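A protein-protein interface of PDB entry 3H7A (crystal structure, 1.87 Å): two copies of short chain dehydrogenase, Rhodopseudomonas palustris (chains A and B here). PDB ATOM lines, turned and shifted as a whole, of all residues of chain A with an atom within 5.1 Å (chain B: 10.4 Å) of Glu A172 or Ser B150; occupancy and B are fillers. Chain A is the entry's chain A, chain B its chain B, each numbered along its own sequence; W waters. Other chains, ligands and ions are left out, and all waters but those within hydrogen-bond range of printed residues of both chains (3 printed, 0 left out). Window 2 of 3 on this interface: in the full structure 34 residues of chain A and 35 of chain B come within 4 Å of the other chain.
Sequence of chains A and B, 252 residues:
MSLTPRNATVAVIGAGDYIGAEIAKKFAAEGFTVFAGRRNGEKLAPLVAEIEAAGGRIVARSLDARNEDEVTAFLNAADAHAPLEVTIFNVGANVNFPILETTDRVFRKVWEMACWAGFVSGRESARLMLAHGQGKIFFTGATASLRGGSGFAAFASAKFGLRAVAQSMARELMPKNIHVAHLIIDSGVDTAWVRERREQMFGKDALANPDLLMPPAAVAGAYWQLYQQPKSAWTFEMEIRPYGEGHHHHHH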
ATOM      1  N   SER A 168       2.516   6.009 -29.042  1.00  0.00           N
ATOM      2  CA  SER A 168       1.727   5.092 -28.212  1.00  0.00           C
ATOM      3  C   SER A 168       0.851   4.146 -29.008  1.00  0.00           C
ATOM      4  O   SER A 168       0.770   2.957 -28.709  1.00  0.00           O
ATOM      5  CB  SER A 168       0.866   5.890 -27.254  1.00  0.00           C
ATOM      6  OG  SER A 168       1.723   6.652 -26.414  1.00  0.00           O
ATOM      7  N   MET A 169       0.198   4.678 -30.031  1.00  0.00           N
ATOM      8  CA  MET A 169      -0.632   3.850 -30.887  1.00  0.00           C
ATOM      9  C   MET A 169       0.237   2.811 -31.589  1.00  0.00           C
ATOM     10  O   MET A 169      -0.154   1.651 -31.691  1.00  0.00           O
ATOM     11  CB  MET A 169      -1.367   4.725 -31.904  1.00  0.00           C
ATOM     12  CG  MET A 169      -2.671   5.352 -31.357  1.00  0.00           C
ATOM     13  SD  MET A 169      -3.538   6.341 -32.640  1.00  0.00           S
ATOM     14  CE  MET A 169      -3.831   5.060 -33.840  1.00  0.00           C
ATOM     15  N   ALA A 170       1.417   3.229 -32.060  1.00  0.00           N
ATOM     16  CA  ALA A 170       2.349   2.309 -32.740  1.00  0.00           C
ATOM     17  C   ALA A 170       2.808   1.190 -31.818  1.00  0.00           C
ATOM     18  O   ALA A 170       2.801   0.020 -32.206  1.00  0.00           O
ATOM     19  CB  ALA A 170       3.565   3.059 -33.312  1.00  0.00           C
ATOM     20  N   ARG A 171       3.195   1.540 -30.597  1.00  0.00           N
ATOM     21  CA  ARG A 171       3.636   0.516 -29.649  1.00  0.00           C
ATOM     22  C   ARG A 171       2.576  -0.570 -29.443  1.00  0.00           C
ATOM     23  O   ARG A 171       2.895  -1.753 -29.411  1.00  0.00           O
ATOM     24  CB  ARG A 171       4.003   1.120 -28.279  1.00  0.00           C
ATOM     25  CG  ARG A 171       5.158   2.128 -28.241  1.00  0.00           C
ATOM     26  CD  ARG A 171       6.512   1.570 -28.616  1.00  0.00           C
ATOM     27  NE  ARG A 171       6.952   0.498 -27.729  1.00  0.00           N
ATOM     28  CZ  ARG A 171       8.157  -0.070 -27.775  1.00  0.00           C
ATOM     29  NH1 ARG A 171       8.449  -1.050 -26.927  1.00  0.00           N
ATOM     30  NH2 ARG A 171       9.068   0.337 -28.661  1.00  0.00           N
ATOM     31  N   GLU A 172       1.316  -0.160 -29.321  1.00  0.00           N
ATOM     32  CA  GLU A 172       0.215  -1.077 -29.046  1.00  0.00           C
ATOM     33  C   GLU A 172      -0.247  -1.850 -30.278  1.00  0.00           C
ATOM     34  O   GLU A 172      -0.567  -3.037 -30.187  1.00  0.00           O
ATOM     35  CB  GLU A 172      -0.967  -0.305 -28.428  1.00  0.00           C
ATOM     36  CG  GLU A 172      -2.277  -1.096 -28.377  1.00  0.00           C
ATOM     37  CD  GLU A 172      -3.427  -0.401 -27.665  1.00  0.00           C
ATOM     38  OE1 GLU A 172      -3.298   0.784 -27.254  1.00  0.00           O
ATOM     39  OE2 GLU A 172      -4.472  -1.072 -27.509  1.00  0.00           O
ATOM     40  N   LEU A 173      -0.274  -1.182 -31.427  1.00  0.00           N
ATOM     41  CA  LEU A 173      -1.016  -1.678 -32.579  1.00  0.00           C
ATOM     42  C   LEU A 173      -0.189  -2.307 -33.690  1.00  0.00           C
ATOM     43  O   LEU A 173      -0.740  -3.063 -34.488  1.00  0.00           O
ATOM     44  CB  LEU A 173      -1.889  -0.571 -33.182  1.00  0.00           C
ATOM     45  CG  LEU A 173      -3.052   0.021 -32.377  1.00  0.00           C
ATOM     46  CD1 LEU A 173      -3.647   1.123 -33.199  1.00  0.00           C
ATOM     47  CD2 LEU A 173      -4.117  -1.016 -32.012  1.00  0.00           C
ATOM     48  N   MET A 174       1.110  -2.008 -33.768  1.00  0.00           N
ATOM     49  CA  MET A 174       1.974  -2.713 -34.755  1.00  0.00           C
ATOM     50  C   MET A 174       2.028  -4.221 -34.529  1.00  0.00           C
ATOM     51  O   MET A 174       1.922  -4.968 -35.504  1.00  0.00           O
ATOM     52  CB  MET A 174       3.379  -2.116 -34.878  1.00  0.00           C
ATOM     53  CG  MET A 174       3.320  -0.644 -35.028  1.00  0.00           C
ATOM     54  SD  MET A 174       4.189  -0.073 -36.426  1.00  0.00           S
ATOM     55  CE  MET A 174       5.654   0.076 -35.710  1.00  0.00           C
ATOM     56  N   PRO A 175       2.173  -4.679 -33.261  1.00  0.00           N
ATOM     57  CA  PRO A 175       1.981  -6.102 -33.024  1.00  0.00           C
ATOM     58  C   PRO A 175       0.611  -6.669 -33.420  1.00  0.00           C
ATOM     59  O   PRO A 175       0.472  -7.886 -33.524  1.00  0.00           O
ATOM     60  CB  PRO A 175       2.139  -6.213 -31.505  1.00  0.00           C
ATOM     61  CG  PRO A 175       3.055  -5.114 -31.149  1.00  0.00           C
ATOM     62  CD  PRO A 175       2.570  -3.995 -32.008  1.00  0.00           C
ATOM     63  N   LYS A 176      -0.389  -5.811 -33.610  1.00  0.00           N
ATOM     64  CA  LYS A 176      -1.739  -6.245 -33.943  1.00  0.00           C
ATOM     65  C   LYS A 176      -2.070  -5.926 -35.400  1.00  0.00           C
ATOM     66  O   LYS A 176      -3.242  -5.794 -35.756  1.00  0.00           O
ATOM     67  CB  LYS A 176      -2.766  -5.612 -32.994  1.00  0.00           C
ATOM     68  CG  LYS A 176      -2.725  -6.173 -31.566  1.00  0.00           C
ATOM     69  CD  LYS A 176      -3.681  -5.425 -30.648  1.00  0.00           C
ATOM     70  CE  LYS A 176      -3.770  -6.082 -29.283  1.00  0.00           C
ATOM     71  NZ  LYS A 176      -2.570  -5.754 -28.477  1.00  0.00           N
ATOM     72  N   ASN B  94      -0.376  10.569 -14.258  1.00  0.00           N
ATOM     73  CA  ASN B  94      -0.017   9.282 -14.868  1.00  0.00           C
ATOM     74  C   ASN B  94      -1.214   8.330 -14.951  1.00  0.00           C
ATOM     75  O   ASN B  94      -1.697   7.843 -13.931  1.00  0.00           O
ATOM     76  CB  ASN B  94       1.174   8.624 -14.160  1.00  0.00           C
ATOM     77  CG  ASN B  94       1.860   7.555 -15.026  1.00  0.00           C
ATOM     78  OD1 ASN B  94       1.203   6.758 -15.701  1.00  0.00           O
ATOM     79  ND2 ASN B  94       3.191   7.540 -15.003  1.00  0.00           N
ATOM     80  N   VAL B  95      -1.709   8.123 -16.175  1.00  0.00           N
ATOM     81  CA  VAL B  95      -2.795   7.173 -16.461  1.00  0.00           C
ATOM     82  C   VAL B  95      -2.481   6.357 -17.705  1.00  0.00           C
ATOM     83  O   VAL B  95      -1.788   6.829 -18.606  1.00  0.00           O
ATOM     84  CB  VAL B  95      -4.182   7.865 -16.641  1.00  0.00           C
ATOM     85  CG1 VAL B  95      -4.641   8.509 -15.341  1.00  0.00           C
ATOM     86  CG2 VAL B  95      -4.172   8.894 -17.767  1.00  0.00           C
ATOM     87  N   ASN B  96      -2.999   5.134 -17.758  1.00  0.00           N
ATOM     88  CA  ASN B  96      -2.730   4.234 -18.863  1.00  0.00           C
ATOM     89  C   ASN B  96      -4.028   3.602 -19.330  1.00  0.00           C
ATOM     90  O   ASN B  96      -4.740   3.015 -18.535  1.00  0.00           O
ATOM     91  CB  ASN B  96      -1.732   3.148 -18.416  1.00  0.00           C
ATOM     92  CG  ASN B  96      -1.273   2.247 -19.564  1.00  0.00           C
ATOM     93  OD1 ASN B  96      -1.994   1.355 -20.002  1.00  0.00           O
ATOM     94  ND2 ASN B  96      -0.055   2.471 -20.038  1.00  0.00           N
ATOM     95  N   PHE B  97      -4.354   3.741 -20.613  1.00  0.00           N
ATOM     96  CA  PHE B  97      -5.491   3.039 -21.181  1.00  0.00           C
ATOM     97  C   PHE B  97      -5.116   2.624 -22.574  1.00  0.00           C
ATOM     98  O   PHE B  97      -4.566   3.434 -23.307  1.00  0.00           O
ATOM     99  CB  PHE B  97      -6.719   3.952 -21.317  1.00  0.00           C
ATOM    100  CG  PHE B  97      -7.296   4.430 -20.025  1.00  0.00           C
ATOM    101  CD1 PHE B  97      -8.269   3.679 -19.363  1.00  0.00           C
ATOM    102  CD2 PHE B  97      -6.900   5.659 -19.485  1.00  0.00           C
ATOM    103  CE1 PHE B  97      -8.824   4.123 -18.168  1.00  0.00           C
ATOM    104  CE2 PHE B  97      -7.446   6.110 -18.281  1.00  0.00           C
ATOM    105  CZ  PHE B  97      -8.407   5.339 -17.624  1.00  0.00           C
ATOM    106  N   PRO B  98      -5.443   1.384 -22.970  1.00  0.00           N
ATOM    107  CA  PRO B  98      -5.351   1.023 -24.385  1.00  0.00           C
ATOM    108  C   PRO B  98      -6.046   2.055 -25.267  1.00  0.00           C
ATOM    109  O   PRO B  98      -6.956   2.745 -24.809  1.00  0.00           O
ATOM    110  CB  PRO B  98      -6.107  -0.301 -24.461  1.00  0.00           C
ATOM    111  CG  PRO B  98      -5.903  -0.913 -23.114  1.00  0.00           C
ATOM    112  CD  PRO B  98      -5.895   0.256 -22.134  1.00  0.00           C
ATOM    113  N   ILE B  99      -5.637   2.151 -26.528  1.00  0.00           N
ATOM    114  CA  ILE B  99      -6.138   3.235 -27.371  1.00  0.00           C
ATOM    115  C   ILE B  99      -7.679   3.266 -27.489  1.00  0.00           C
ATOM    116  O   ILE B  99      -8.306   4.323 -27.337  1.00  0.00           O
ATOM    117  CB  ILE B  99      -5.400   3.295 -28.727  1.00  0.00           C
ATOM    118  CG1 ILE B  99      -5.827   4.530 -29.518  1.00  0.00           C
ATOM    119  CG2 ILE B  99      -5.593   2.016 -29.530  1.00  0.00           C
ATOM    120  CD1 ILE B  99      -5.436   5.861 -28.829  1.00  0.00           C
ATOM    121  N   LEU B 100      -8.292   2.101 -27.678  1.00  0.00           N
ATOM    122  CA  LEU B 100      -9.750   2.007 -27.811  1.00  0.00           C
ATOM    123  C   LEU B 100     -10.483   2.295 -26.495  1.00  0.00           C
ATOM    124  O   LEU B 100     -11.675   2.558 -26.495  1.00  0.00           O
ATOM    125  CB  LEU B 100     -10.159   0.646 -28.401  1.00  0.00           C
ATOM    126  CG  LEU B 100      -9.620   0.352 -29.805  1.00  0.00           C
ATOM    127  CD1 LEU B 100     -10.272  -0.890 -30.435  1.00  0.00           C
ATOM    128  CD2 LEU B 100      -9.803   1.557 -30.706  1.00  0.00           C
ATOM    129  N   GLU B 101      -9.752   2.280 -25.383  1.00  0.00           N
ATOM    130  CA  GLU B 101     -10.320   2.552 -24.076  1.00  0.00           C
ATOM    131  C   GLU B 101      -9.902   3.923 -23.577  1.00  0.00           C
ATOM    132  O   GLU B 101     -10.079   4.248 -22.400  1.00  0.00           O
ATOM    133  CB  GLU B 101      -9.888   1.477 -23.084  1.00  0.00           C
ATOM    134  CG  GLU B 101     -10.370   0.075 -23.471  1.00  0.00           C
ATOM    135  CD  GLU B 101      -9.752  -1.015 -22.613  1.00  0.00           C
ATOM    136  OE1 GLU B 101      -9.437  -0.738 -21.436  1.00  0.00           O
ATOM    137  OE2 GLU B 101      -9.574  -2.149 -23.118  1.00  0.00           O
ATOM    138  N   THR B 102      -9.362   4.744 -24.472  1.00  0.00           N
ATOM    139  CA  THR B 102      -8.972   6.097 -24.080  1.00  0.00           C
ATOM    140  C   THR B 102     -10.118   6.994 -24.535  1.00  0.00           C
ATOM    141  O   THR B 102     -10.294   7.238 -25.723  1.00  0.00           O
ATOM    142  CB  THR B 102      -7.590   6.510 -24.707  1.00  0.00           C
ATOM    143  OG1 THR B 102      -6.561   5.583 -24.311  1.00  0.00           O
ATOM    144  CG2 THR B 102      -7.189   7.906 -24.295  1.00  0.00           C
ATOM    145  N   ALA B 144       7.301   9.937 -20.077  1.00  0.00           N
ATOM    146  CA  ALA B 144       6.235  10.099 -21.060  1.00  0.00           C
ATOM    147  C   ALA B 144       6.342  11.457 -21.772  1.00  0.00           C
ATOM    148  O   ALA B 144       5.683  11.654 -22.776  1.00  0.00           O
ATOM    149  CB  ALA B 144       4.863   9.915 -20.429  1.00  0.00           C
ATOM    150  N   ARG B 147       9.011   9.715 -24.738  1.00  0.00           N
ATOM    151  CA  ARG B 147       8.523   8.613 -25.578  1.00  0.00           C
ATOM    152  C   ARG B 147       7.137   8.138 -25.146  1.00  0.00           C
ATOM    153  O   ARG B 147       6.816   8.121 -23.966  1.00  0.00           O
ATOM    154  CB  ARG B 147       9.517   7.449 -25.618  1.00  0.00           C
ATOM    155  CG  ARG B 147       9.889   6.889 -24.280  1.00  0.00           C
ATOM    156  CD  ARG B 147      11.200   6.122 -24.372  1.00  0.00           C
ATOM    157  NE  ARG B 147      11.907   6.185 -23.094  1.00  0.00           N
ATOM    158  CZ  ARG B 147      12.880   7.049 -22.802  1.00  0.00           C
ATOM    159  NH1 ARG B 147      13.308   7.931 -23.702  1.00  0.00           N
ATOM    160  NH2 ARG B 147      13.436   7.020 -21.600  1.00  0.00           N
ATOM    161  N   GLY B 148       6.310   7.755 -26.111  1.00  0.00           N
ATOM    162  CA  GLY B 148       4.970   7.277 -25.810  1.00  0.00           C
ATOM    163  C   GLY B 148       4.849   5.763 -25.888  1.00  0.00           C
ATOM    164  O   GLY B 148       4.869   5.192 -26.969  1.00  0.00           O
ATOM    165  N   GLY B 149       4.717   5.115 -24.742  1.00  0.00           N
ATOM    166  CA  GLY B 149       4.558   3.665 -24.709  1.00  0.00           C
ATOM    167  C   GLY B 149       3.127   3.224 -24.918  1.00  0.00           C
ATOM    168  O   GLY B 149       2.225   4.053 -25.043  1.00  0.00           O
ATOM    169  N   SER B 150       2.920   1.912 -24.947  1.00  0.00           N
ATOM    170  CA  SER B 150       1.595   1.348 -25.125  1.00  0.00           C
ATOM    171  C   SER B 150       0.695   1.705 -23.944  1.00  0.00           C
ATOM    172  O   SER B 150       1.034   1.472 -22.778  1.00  0.00           O
ATOM    173  CB  SER B 150       1.691  -0.165 -25.288  1.00  0.00           C
ATOM    174  OG  SER B 150       0.412  -0.753 -25.390  1.00  0.00           O
ATOM    175  N   GLY B 151      -0.452   2.293 -24.256  1.00  0.00           N
ATOM    176  CA  GLY B 151      -1.437   2.636 -23.241  1.00  0.00           C
ATOM    177  C   GLY B 151      -1.309   4.091 -22.822  1.00  0.00           C
ATOM    178  O   GLY B 151      -2.165   4.611 -22.104  1.00  0.00           O
ATOM    179  N   PHE B 152      -0.247   4.754 -23.278  1.00  0.00           N
ATOM    180  CA  PHE B 152       0.060   6.107 -22.803  1.00  0.00           C
ATOM    181  C   PHE B 152      -0.330   7.250 -23.741  1.00  0.00           C
ATOM    182  O   PHE B 152       0.166   8.375 -23.557  1.00  0.00           O
ATOM    183  CB  PHE B 152       1.543   6.199 -22.446  1.00  0.00           C
ATOM    184  CG  PHE B 152       1.898   5.490 -21.178  1.00  0.00           C
ATOM    185  CD1 PHE B 152       1.408   5.939 -19.966  1.00  0.00           C
ATOM    186  CD2 PHE B 152       2.726   4.384 -21.202  1.00  0.00           C
ATOM    187  CE1 PHE B 152       1.721   5.279 -18.786  1.00  0.00           C
ATOM    188  CE2 PHE B 152       3.058   3.714 -20.024  1.00  0.00           C
ATOM    189  CZ  PHE B 152       2.554   4.161 -18.819  1.00  0.00           C
ATOM    190  N   ALA B 153      -1.211   6.998 -24.717  1.00  0.00           N
ATOM    191  CA  ALA B 153      -1.562   8.054 -25.695  1.00  0.00           C
ATOM    192  C   ALA B 153      -2.054   9.362 -25.085  1.00  0.00           C
ATOM    193  O   ALA B 153      -1.626  10.432 -25.522  1.00  0.00           O
ATOM    194  CB  ALA B 153      -2.543   7.545 -26.779  1.00  0.00           C
ATOM    195  N   ALA B 154      -2.913   9.294 -24.067  1.00  0.00           N
ATOM    196  CA  ALA B 154      -3.407  10.529 -23.454  1.00  0.00           C
ATOM    197  C   ALA B 154      -2.339  11.243 -22.628  1.00  0.00           C
ATOM    198  O   ALA B 154      -2.175  12.458 -22.745  1.00  0.00           O
ATOM    199  CB  ALA B 154      -4.673  10.283 -22.617  1.00  0.00           C
ATOM    200  N   PHE B 155      -1.649  10.493 -21.772  1.00  0.00           N
ATOM    201  CA  PHE B 155      -0.630  11.069 -20.891  1.00  0.00           C
ATOM    202  C   PHE B 155       0.610  11.589 -21.640  1.00  0.00           C
ATOM    203  O   PHE B 155       1.057  12.719 -21.406  1.00  0.00           O
ATOM    204  CB  PHE B 155      -0.242  10.045 -19.815  1.00  0.00           C
ATOM    205  CG  PHE B 155       0.675  10.582 -18.744  1.00  0.00           C
ATOM    206  CD1 PHE B 155       0.360  11.736 -18.042  1.00  0.00           C
ATOM    207  CD2 PHE B 155       1.858   9.920 -18.430  1.00  0.00           C
ATOM    208  CE1 PHE B 155       1.216  12.227 -17.041  1.00  0.00           C
ATOM    209  CE2 PHE B 155       2.722  10.405 -17.432  1.00  0.00           C
ATOM    210  CZ  PHE B 155       2.389  11.556 -16.729  1.00  0.00           C
ATOM    211  N   ALA B 156       1.162  10.775 -22.542  1.00  0.00           N
ATOM    212  CA  ALA B 156       2.317  11.170 -23.318  1.00  0.00           C
ATOM    213  C   ALA B 156       1.966  12.364 -24.223  1.00  0.00           C
ATOM    214  O   ALA B 156       2.794  13.256 -24.406  1.00  0.00           O
ATOM    215  CB  ALA B 156       2.849   9.997 -24.146  1.00  0.00           C
HETATM  216  O   HOH W   1       5.295   0.249 -24.717  1.00  0.00           O
HETATM  217  O   HOH W   2      -1.420   2.532 -26.837  1.00  0.00           O
HETATM  218  O   HOH W   3      -7.203  -1.051 -27.702  1.00  0.00           O
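The side-chain hydroxyl (OG) of Ser A168 is in hydrogen-bond range of the backbone NH (N) of Ala B153 (3.4 Å). The backbone NH of Ser A168 is in hydrogen-bond range of the backbone carbonyl oxygen of Gly B148. The side-chain hydroxyl (OG) of Ser A168 sits at hydrogen-bond distance from the backbone carbonyl oxygen (O) of Gly B149. The side-chain carboxylate (OE1) of Glu A172 sits at hydrogen-bond distance from the backbone NH (N) of Ile B99 (2.8 Å).
The backbone carbonyl oxygen of Pro B98 lies within hydrogen-bond range of the side-chain hydroxyl of Thr B102, at 2.9 Å. O of Ser B150 sits at hydrogen-bond distance from ND2 of Asn B96, 3.1 Å away.
Among the printed residues, merely in contact across the chains: Arg A171 with Gly B148, Glu A172 with Ser B150, Ser A168 with Phe B152, Glu A172 with Pro B98, Arg A171 with Ser B150, Met A169 with Ile B99 and Arg A171 with Gly B149.
Of the printed residues of chain B, Ser A168 touches Gly B148, Gly B149, Phe B152 and Ala B153. Ala A170 touches none of the printed residues of chain B. Glu A172 touches just these residues of chain B: Pro B98 (3.5 Å), Ile B99 (2.8 Å) and Ser B150 (3.4 Å). Leu A173 touches none of the printed residues of chain B. Glu B101 touches none of the printed residues of chain A. Of the printed residues of chain A, Gly B148 touches Ser A168 (3.2 Å) and Arg A171 (3.3 Å). Printed residues of chain A within 4 Å of Ser B150: Arg A171 (3.6 Å) and Glu A172 (3.4 Å). Printed residues of chain A within 4 Å of Phe B152: Ser A168 (3.4 Å). The nearest residue of chain B that does not touch Glu A172 is Gly B151 (4.4 Å). The nearest printed residue of chain A that does not touch Ser B150 is Ser A168 (4.01 Å). The nearest printed residue of chain A that does not touch Phe B152 is Glu A172 (6.4 Å).
Printed residues of chain B that touch a printed residue of chain A: Pro B98, Ile B99, Gly B148, Gly B149, Ser B150, Phe B152 and Ala B153. Hydrophobic or aromatic side chains of chain B that line the printed part of chain A: Pro B98, Ile B99, Phe B152 and Ala B153.
No position is printed for both chains. Of the 11 pairs that touch across the chains among the printed residues, none has its exchanged pair printed and touching as well.
Water W2 lies within hydrogen-bond range of OE1 of Glu A172 (2.6 Å), N of Gly B151 (2.8 Å) and O of Ser A168 (2.9 Å). Water W3 lies within hydrogen-bond range of the side-chain carboxylate of Glu A172 and the backbone NH of Leu B100. Water W1 bridges the backbone NH of Ser B150 (2.9 Å) and the guanidinium group of Arg A171 (3.4 Å).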
